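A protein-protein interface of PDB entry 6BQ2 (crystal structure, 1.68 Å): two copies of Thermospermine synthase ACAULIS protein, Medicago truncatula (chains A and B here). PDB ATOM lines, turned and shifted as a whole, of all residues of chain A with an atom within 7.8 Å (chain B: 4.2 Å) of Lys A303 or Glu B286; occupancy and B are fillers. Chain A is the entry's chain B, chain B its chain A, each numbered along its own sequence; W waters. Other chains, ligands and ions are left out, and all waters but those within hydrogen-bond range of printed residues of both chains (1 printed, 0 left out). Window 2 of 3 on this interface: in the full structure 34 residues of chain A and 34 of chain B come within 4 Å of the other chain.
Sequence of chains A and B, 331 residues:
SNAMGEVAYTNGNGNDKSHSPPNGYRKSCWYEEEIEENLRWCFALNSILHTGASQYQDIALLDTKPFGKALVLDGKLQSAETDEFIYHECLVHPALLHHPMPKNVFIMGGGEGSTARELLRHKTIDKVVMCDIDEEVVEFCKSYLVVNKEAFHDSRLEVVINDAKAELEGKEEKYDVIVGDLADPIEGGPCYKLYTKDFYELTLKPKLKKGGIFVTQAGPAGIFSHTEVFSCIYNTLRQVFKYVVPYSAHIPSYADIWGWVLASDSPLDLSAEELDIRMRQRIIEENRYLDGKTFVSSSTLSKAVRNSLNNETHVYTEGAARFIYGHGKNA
The side-chain hydroxyl of Thr B294 is in hydrogen-bond range of the guanidinium group of Arg A306 (3.4 Å).
OG1 of Thr B294 is in hydrogen-bond range of N of Lys A303, 3.0 Å away.
The backbone carbonyl oxygen (O) of Asn B287 sits at hydrogen-bond distance from the side-chain amino group (NZ) of Lys A303 (2.8 Å).
OE1 of Glu B286 is in salt-bridge range of NZ of Lys A303.
The guanidinium group (NH1) of Arg A306 lies within salt-bridge range of the side-chain carboxylate (OD2) of Asp B291.
The backbone carbonyl oxygen (O) of Arg A306 lies within hydrogen-bond range of the side-chain amide nitrogen (ND2) of Asn A310 (3.2 Å).
NH1 of Arg B121 lies within hydrogen-bond range of OD1 of Asn B287 (2.9 Å).
O of Lys A303 lies close to OD1 of Asn A307, at 3.4 Å.
The backbone carbonyl oxygen of Leu A301 sits at hydrogen-bond distance from the guanidinium group of Arg A306, 2.8 Å away.
The side-chain hydroxyl of Thr B294 sits at hydrogen-bond distance from the side-chain carboxylate of Asp B291.
Among the printed residues, pairs that only touch across the chains: Ser A302 with Tyr B289 (3.7 Å), Ser A302 with Thr B294 (3.4 Å), Lys A303 with Tyr B289 (3.3 Å), Lys A303 with Asp B291 (3.6 Å) and Ala A304 with Arg B288 (3.95 Å).
Of chain B, only Glu B286, Asn B287, Tyr B289, Asp B291 and Thr B294 come within 4 Å of Lys A303.
Of the printed residues of chain B, Ala A304 touches Arg B288 (3.95 Å).
Printed residues of chain B within 4 Å of Arg A306: Asp B291 and Thr B294.
Printed residues of chain A within 4 Å of Glu B286: Lys A303.
Of the printed residues of chain A, Asn B287 touches Lys A303.
Of the printed residues of chain A, Tyr B289 touches Ser A302 (3.7 Å) and Lys A303 (3.3 Å).
Printed residues of chain A within 4 Å of Thr B294: Ser A302 (3.4 Å), Lys A303 (3.0 Å) and Arg A306 (3.4 Å).
The nearest residue of chain A that does not touch Glu B286 is Asn A307 (6.9 Å).
Of the 12 printed residues of chain A, 4 touch a printed residue of chain B.
Printed residues of chain A that touch a printed residue of chain B: Ser A302, Lys A303, Ala A304 and Arg A306.
Among the printed residues, 10 pairs touch across the chains.
No position is printed for both chains.
Water W1 lies within hydrogen-bond range of OG of Ser A302 (2.8 Å), N of Ala A304 (2.8 Å), O of Tyr B289 (2.8 Å) and N of Lys A303 (3.3 Å).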
ATOM      1  N   ILE A 223      -5.877 -13.069 -24.595  1.00  0.00           N
ATOM      2  CA  ILE A 223      -5.792 -11.687 -24.077  1.00  0.00           C
ATOM      3  C   ILE A 223      -4.726 -11.544 -22.982  1.00  0.00           C
ATOM      4  O   ILE A 223      -4.035 -10.520 -22.945  1.00  0.00           O
ATOM      5  CB  ILE A 223      -7.189 -11.177 -23.630  1.00  0.00           C
ATOM      6  CG1 ILE A 223      -7.150  -9.759 -23.033  1.00  0.00           C
ATOM      7  CG2 ILE A 223      -7.827 -12.094 -22.602  1.00  0.00           C
ATOM      8  CD1 ILE A 223      -6.820  -8.755 -24.076  1.00  0.00           C
ATOM      9  N   THR A 300      -5.425  -9.116 -37.526  1.00  0.00           N
ATOM     10  CA  THR A 300      -5.834  -7.904 -36.869  1.00  0.00           C
ATOM     11  C   THR A 300      -6.028  -8.272 -35.420  1.00  0.00           C
ATOM     12  O   THR A 300      -7.094  -8.755 -35.020  1.00  0.00           O
ATOM     13  CB  THR A 300      -7.161  -7.375 -37.456  1.00  0.00           C
ATOM     14  OG1 THR A 300      -7.059  -7.244 -38.869  1.00  0.00           O
ATOM     15  CG2 THR A 300      -7.503  -6.013 -36.872  1.00  0.00           C
ATOM     16  N   LEU A 301      -5.023  -8.019 -34.620  1.00  0.00           N
ATOM     17  CA  LEU A 301      -5.065  -8.384 -33.209  1.00  0.00           C
ATOM     18  C   LEU A 301      -5.891  -7.333 -32.433  1.00  0.00           C
ATOM     19  O   LEU A 301      -6.134  -6.215 -32.917  1.00  0.00           O
ATOM     20  CB  LEU A 301      -3.654  -8.463 -32.642  1.00  0.00           C
ATOM     21  CG  LEU A 301      -2.755  -9.434 -33.426  1.00  0.00           C
ATOM     22  CD1 LEU A 301      -1.396  -9.464 -32.835  1.00  0.00           C
ATOM     23  CD2 LEU A 301      -3.374 -10.826 -33.520  1.00  0.00           C
ATOM     24  N   SER A 302      -6.293  -7.683 -31.219  1.00  0.00           N
ATOM     25  CA  SER A 302      -7.078  -6.762 -30.402  1.00  0.00           C
ATOM     26  C   SER A 302      -6.211  -5.646 -29.861  1.00  0.00           C
ATOM     27  O   SER A 302      -4.996  -5.736 -29.866  1.00  0.00           O
ATOM     28  CB  SER A 302      -7.773  -7.470 -29.229  1.00  0.00           C
ATOM     29  OG  SER A 302      -6.860  -7.789 -28.194  1.00  0.00           O
ATOM     30  N   LYS A 303      -6.859  -4.596 -29.363  1.00  0.00           N
ATOM     31  CA  LYS A 303      -6.140  -3.419 -28.875  1.00  0.00           C
ATOM     32  C   LYS A 303      -5.004  -3.760 -27.920  1.00  0.00           C
ATOM     33  O   LYS A 303      -3.858  -3.262 -28.055  1.00  0.00           O
ATOM     34  CB  LYS A 303      -7.140  -2.470 -28.201  1.00  0.00           C
ATOM     35  CG  LYS A 303      -6.537  -1.153 -27.699  1.00  0.00           C
ATOM     36  CD  LYS A 303      -7.577  -0.335 -26.948  1.00  0.00           C
ATOM     37  CE  LYS A 303      -7.007   1.011 -26.532  1.00  0.00           C
ATOM     38  NZ  LYS A 303      -8.040   1.822 -25.890  1.00  0.00           N
ATOM     39  N   ALA A 304      -5.330  -4.568 -26.921  1.00  0.00           N
ATOM     40  CA  ALA A 304      -4.410  -4.820 -25.852  1.00  0.00           C
ATOM     41  C   ALA A 304      -3.287  -5.705 -26.341  1.00  0.00           C
ATOM     42  O   ALA A 304      -2.162  -5.519 -25.946  1.00  0.00           O
ATOM     43  CB  ALA A 304      -5.120  -5.430 -24.684  1.00  0.00           C
ATOM     44  N   VAL A 305      -3.588  -6.655 -27.233  1.00  0.00           N
ATOM     45  CA  VAL A 305      -2.561  -7.570 -27.719  1.00  0.00           C
ATOM     46  C   VAL A 305      -1.609  -6.836 -28.661  1.00  0.00           C
ATOM     47  O   VAL A 305      -0.383  -6.992 -28.592  1.00  0.00           O
ATOM     48  CB  VAL A 305      -3.196  -8.800 -28.416  1.00  0.00           C
ATOM     49  CG1 VAL A 305      -2.111  -9.707 -28.959  1.00  0.00           C
ATOM     50  CG2 VAL A 305      -4.022  -9.557 -27.419  1.00  0.00           C
ATOM     51  N   ARG A 306      -2.174  -6.014 -29.535  1.00  0.00           N
ATOM     52  CA  ARG A 306      -1.368  -5.150 -30.417  1.00  0.00           C
ATOM     53  C   ARG A 306      -0.372  -4.271 -29.638  1.00  0.00           C
ATOM     54  O   ARG A 306       0.807  -4.171 -29.960  1.00  0.00           O
ATOM     55  CB  ARG A 306      -2.291  -4.253 -31.233  1.00  0.00           C
ATOM     56  CG  ARG A 306      -1.920  -4.165 -32.669  1.00  0.00           C
ATOM     57  CD  ARG A 306      -2.895  -3.339 -33.495  1.00  0.00           C
ATOM     58  NE  ARG A 306      -4.297  -3.726 -33.315  1.00  0.00           N
ATOM     59  CZ  ARG A 306      -5.264  -2.940 -32.862  1.00  0.00           C
ATOM     60  NH1 ARG A 306      -5.053  -1.654 -32.571  1.00  0.00           N
ATOM     61  NH2 ARG A 306      -6.486  -3.452 -32.695  1.00  0.00           N
ATOM     62  N   ASN A 307      -0.861  -3.648 -28.593  1.00  0.00           N
ATOM     63  CA  ASN A 307      -0.033  -2.708 -27.833  1.00  0.00           C
ATOM     64  C   ASN A 307       1.062  -3.448 -27.039  1.00  0.00           C
ATOM     65  O   ASN A 307       2.234  -3.000 -26.923  1.00  0.00           O
ATOM     66  CB  ASN A 307      -0.936  -1.842 -26.937  1.00  0.00           C
ATOM     67  CG  ASN A 307      -1.832  -0.861 -27.744  1.00  0.00           C
ATOM     68  OD1 ASN A 307      -1.749  -0.764 -28.979  1.00  0.00           O
ATOM     69  ND2 ASN A 307      -2.705  -0.140 -27.036  1.00  0.00           N
ATOM     70  N   SER A 308       0.687  -4.613 -26.535  1.00  0.00           N
ATOM     71  CA  SER A 308       1.569  -5.466 -25.769  1.00  0.00           C
ATOM     72  C   SER A 308       2.713  -5.982 -26.647  1.00  0.00           C
ATOM     73  O   SER A 308       3.891  -5.913 -26.253  1.00  0.00           O
ATOM     74  CB  SER A 308       0.691  -6.521 -25.078  1.00  0.00           C
ATOM     75  OG  SER A 308       1.402  -7.531 -24.455  1.00  0.00           O
ATOM     76  N   LEU A 309       2.394  -6.418 -27.870  1.00  0.00           N
ATOM     77  CA  LEU A 309       3.415  -6.785 -28.872  1.00  0.00           C
ATOM     78  C   LEU A 309       4.274  -5.597 -29.266  1.00  0.00           C
ATOM     79  O   LEU A 309       5.494  -5.716 -29.301  1.00  0.00           O
ATOM     80  CB  LEU A 309       2.782  -7.433 -30.114  1.00  0.00           C
ATOM     81  CG  LEU A 309       2.806  -8.950 -30.077  1.00  0.00           C
ATOM     82  CD1 LEU A 309       2.054  -9.565 -28.922  1.00  0.00           C
ATOM     83  CD2 LEU A 309       2.236  -9.484 -31.375  1.00  0.00           C
ATOM     84  N   ASN A 310       3.643  -4.450 -29.535  1.00  0.00           N
ATOM     85  CA  ASN A 310       4.380  -3.217 -29.871  1.00  0.00           C
ATOM     86  C   ASN A 310       5.425  -2.841 -28.819  1.00  0.00           C
ATOM     87  O   ASN A 310       6.550  -2.492 -29.171  1.00  0.00           O
ATOM     88  CB  ASN A 310       3.434  -2.017 -30.092  1.00  0.00           C
ATOM     89  CG  ASN A 310       2.908  -1.929 -31.525  1.00  0.00           C
ATOM     90  OD1 ASN A 310       3.645  -2.169 -32.479  1.00  0.00           O
ATOM     91  ND2 ASN A 310       1.628  -1.567 -31.682  1.00  0.00           N
ATOM     92  N   ARG B 121     -20.836   5.110 -19.419  1.00  0.00           N
ATOM     93  CA  ARG B 121     -19.647   5.803 -19.895  1.00  0.00           C
ATOM     94  C   ARG B 121     -19.906   6.691 -21.106  1.00  0.00           C
ATOM     95  O   ARG B 121     -19.061   7.534 -21.438  1.00  0.00           O
ATOM     96  CB  ARG B 121     -18.550   4.794 -20.244  1.00  0.00           C
ATOM     97  CG  ARG B 121     -18.050   4.038 -19.035  1.00  0.00           C
ATOM     98  CD  ARG B 121     -17.028   2.967 -19.413  1.00  0.00           C
ATOM     99  NE  ARG B 121     -15.853   3.576 -20.051  1.00  0.00           N
ATOM    100  CZ  ARG B 121     -15.103   2.992 -20.974  1.00  0.00           C
ATOM    101  NH1 ARG B 121     -15.345   1.766 -21.390  1.00  0.00           N
ATOM    102  NH2 ARG B 121     -14.094   3.653 -21.497  1.00  0.00           N
ATOM    103  N   ARG B 280     -13.348   8.343 -28.868  1.00  0.00           N
ATOM    104  CA  ARG B 280     -12.688   9.479 -28.202  1.00  0.00           C
ATOM    105  C   ARG B 280     -13.684  10.606 -27.886  1.00  0.00           C
ATOM    106  O   ARG B 280     -13.617  11.228 -26.836  1.00  0.00           O
ATOM    107  CB  ARG B 280     -11.518   9.999 -29.051  1.00  0.00           C
ATOM    108  CG  ARG B 280     -10.771  11.196 -28.443  1.00  0.00           C
ATOM    109  CD  ARG B 280      -9.994  10.852 -27.165  1.00  0.00           C
ATOM    110  NE  ARG B 280      -8.848   9.956 -27.408  1.00  0.00           N
ATOM    111  CZ  ARG B 280      -7.595  10.331 -27.741  1.00  0.00           C
ATOM    112  NH1 ARG B 280      -7.254  11.610 -27.904  1.00  0.00           N
ATOM    113  NH2 ARG B 280      -6.665   9.391 -27.926  1.00  0.00           N
ATOM    114  N   GLU B 285     -13.088   8.053 -20.615  1.00  0.00           N
ATOM    115  CA  GLU B 285     -11.931   7.175 -20.379  1.00  0.00           C
ATOM    116  C   GLU B 285     -11.655   6.248 -21.555  1.00  0.00           C
ATOM    117  O   GLU B 285     -12.430   6.209 -22.499  1.00  0.00           O
ATOM    118  CB  GLU B 285     -12.091   6.387 -19.070  1.00  0.00           C
ATOM    119  CG  GLU B 285     -12.112   7.296 -17.838  1.00  0.00           C
ATOM    120  CD  GLU B 285     -12.154   6.531 -16.532  1.00  0.00           C
ATOM    121  OE1 GLU B 285     -12.961   5.589 -16.433  1.00  0.00           O
ATOM    122  OE2 GLU B 285     -11.391   6.868 -15.607  1.00  0.00           O
ATOM    123  N   GLU B 286     -10.561   5.501 -21.488  1.00  0.00           N
ATOM    124  CA  GLU B 286     -10.166   4.608 -22.559  1.00  0.00           C
ATOM    125  C   GLU B 286     -10.778   3.218 -22.397  1.00  0.00           C
ATOM    126  O   GLU B 286     -10.690   2.612 -21.345  1.00  0.00           O
ATOM    127  CB  GLU B 286      -8.645   4.433 -22.573  1.00  0.00           C
ATOM    128  CG  GLU B 286      -7.887   5.642 -23.066  1.00  0.00           C
ATOM    129  CD  GLU B 286      -7.847   5.684 -24.591  1.00  0.00           C
ATOM    130  OE1 GLU B 286      -7.236   4.733 -25.201  1.00  0.00           O
ATOM    131  OE2 GLU B 286      -8.431   6.659 -25.165  1.00  0.00           O
ATOM    132  N   ASN B 287     -11.336   2.669 -23.461  1.00  0.00           N
ATOM    133  CA  ASN B 287     -11.651   1.239 -23.461  1.00  0.00           C
ATOM    134  C   ASN B 287     -10.384   0.399 -23.250  1.00  0.00           C
ATOM    135  O   ASN B 287      -9.280   0.815 -23.640  1.00  0.00           O
ATOM    136  CB  ASN B 287     -12.269   0.803 -24.792  1.00  0.00           C
ATOM    137  CG  ASN B 287     -13.667   1.320 -24.986  1.00  0.00           C
ATOM    138  OD1 ASN B 287     -14.296   1.830 -24.051  1.00  0.00           O
ATOM    139  ND2 ASN B 287     -14.166   1.196 -26.210  1.00  0.00           N
ATOM    140  N   ARG B 288     -10.546  -0.733 -22.564  1.00  0.00           N
ATOM    141  CA  ARG B 288      -9.405  -1.676 -22.343  1.00  0.00           C
ATOM    142  C   ARG B 288      -9.325  -2.719 -23.437  1.00  0.00           C
ATOM    143  O   ARG B 288      -8.216  -3.123 -23.839  1.00  0.00           O
ATOM    144  CB  ARG B 288      -9.527  -2.351 -20.963  1.00  0.00           C
ATOM    145  CG  ARG B 288      -9.618  -1.372 -19.789  1.00  0.00           C
ATOM    146  CD  ARG B 288      -9.191  -1.960 -18.448  1.00  0.00           C
ATOM    147  NE  ARG B 288     -10.248  -2.689 -17.699  1.00  0.00           N
ATOM    148  CZ  ARG B 288     -10.147  -3.915 -17.140  1.00  0.00           C
ATOM    149  NH1 ARG B 288     -11.162  -4.452 -16.470  1.00  0.00           N
ATOM    150  NH2 ARG B 288      -9.010  -4.631 -17.273  1.00  0.00           N
ATOM    151  N   TYR B 289     -10.472  -3.173 -23.953  1.00  0.00           N
ATOM    152  CA  TYR B 289     -10.462  -4.210 -24.988  1.00  0.00           C
ATOM    153  C   TYR B 289     -10.629  -3.684 -26.423  1.00  0.00           C
ATOM    154  O   TYR B 289      -9.914  -4.076 -27.330  1.00  0.00           O
ATOM    155  CB  TYR B 289     -11.567  -5.275 -24.751  1.00  0.00           C
ATOM    156  CG  TYR B 289     -11.480  -6.377 -25.762  1.00  0.00           C
ATOM    157  CD1 TYR B 289     -10.448  -7.313 -25.729  1.00  0.00           C
ATOM    158  CD2 TYR B 289     -12.412  -6.446 -26.796  1.00  0.00           C
ATOM    159  CE1 TYR B 289     -10.391  -8.317 -26.705  1.00  0.00           C
ATOM    160  CE2 TYR B 289     -12.363  -7.405 -27.742  1.00  0.00           C
ATOM    161  CZ  TYR B 289     -11.369  -8.299 -27.731  1.00  0.00           C
ATOM    162  OH  TYR B 289     -11.409  -9.210 -28.767  1.00  0.00           O
ATOM    163  N   ASP B 291     -10.994  -1.311 -29.626  1.00  0.00           N
ATOM    164  CA  ASP B 291     -10.846  -0.173 -30.511  1.00  0.00           C
ATOM    165  C   ASP B 291     -11.487  -0.487 -31.874  1.00  0.00           C
ATOM    166  O   ASP B 291     -12.070  -1.534 -32.062  1.00  0.00           O
ATOM    167  CB  ASP B 291      -9.392   0.292 -30.614  1.00  0.00           C
ATOM    168  CG  ASP B 291      -8.475  -0.736 -31.240  1.00  0.00           C
ATOM    169  OD1 ASP B 291      -8.950  -1.754 -31.796  1.00  0.00           O
ATOM    170  OD2 ASP B 291      -7.249  -0.521 -31.199  1.00  0.00           O
ATOM    171  N   THR B 294     -10.285  -3.594 -33.631  1.00  0.00           N
ATOM    172  CA  THR B 294     -10.766  -4.764 -32.911  1.00  0.00           C
ATOM    173  C   THR B 294     -12.182  -5.087 -33.341  1.00  0.00           C
ATOM    174  O   THR B 294     -12.519  -6.238 -33.614  1.00  0.00           O
ATOM    175  CB  THR B 294     -10.662  -4.623 -31.384  1.00  0.00           C
ATOM    176  OG1 THR B 294      -9.302  -4.298 -31.006  1.00  0.00           O
ATOM    177  CG2 THR B 294     -11.009  -5.924 -30.701  1.00  0.00           C
HETATM  178  O   HOH W   1      -7.812  -5.796 -26.468  1.00  0.00           O
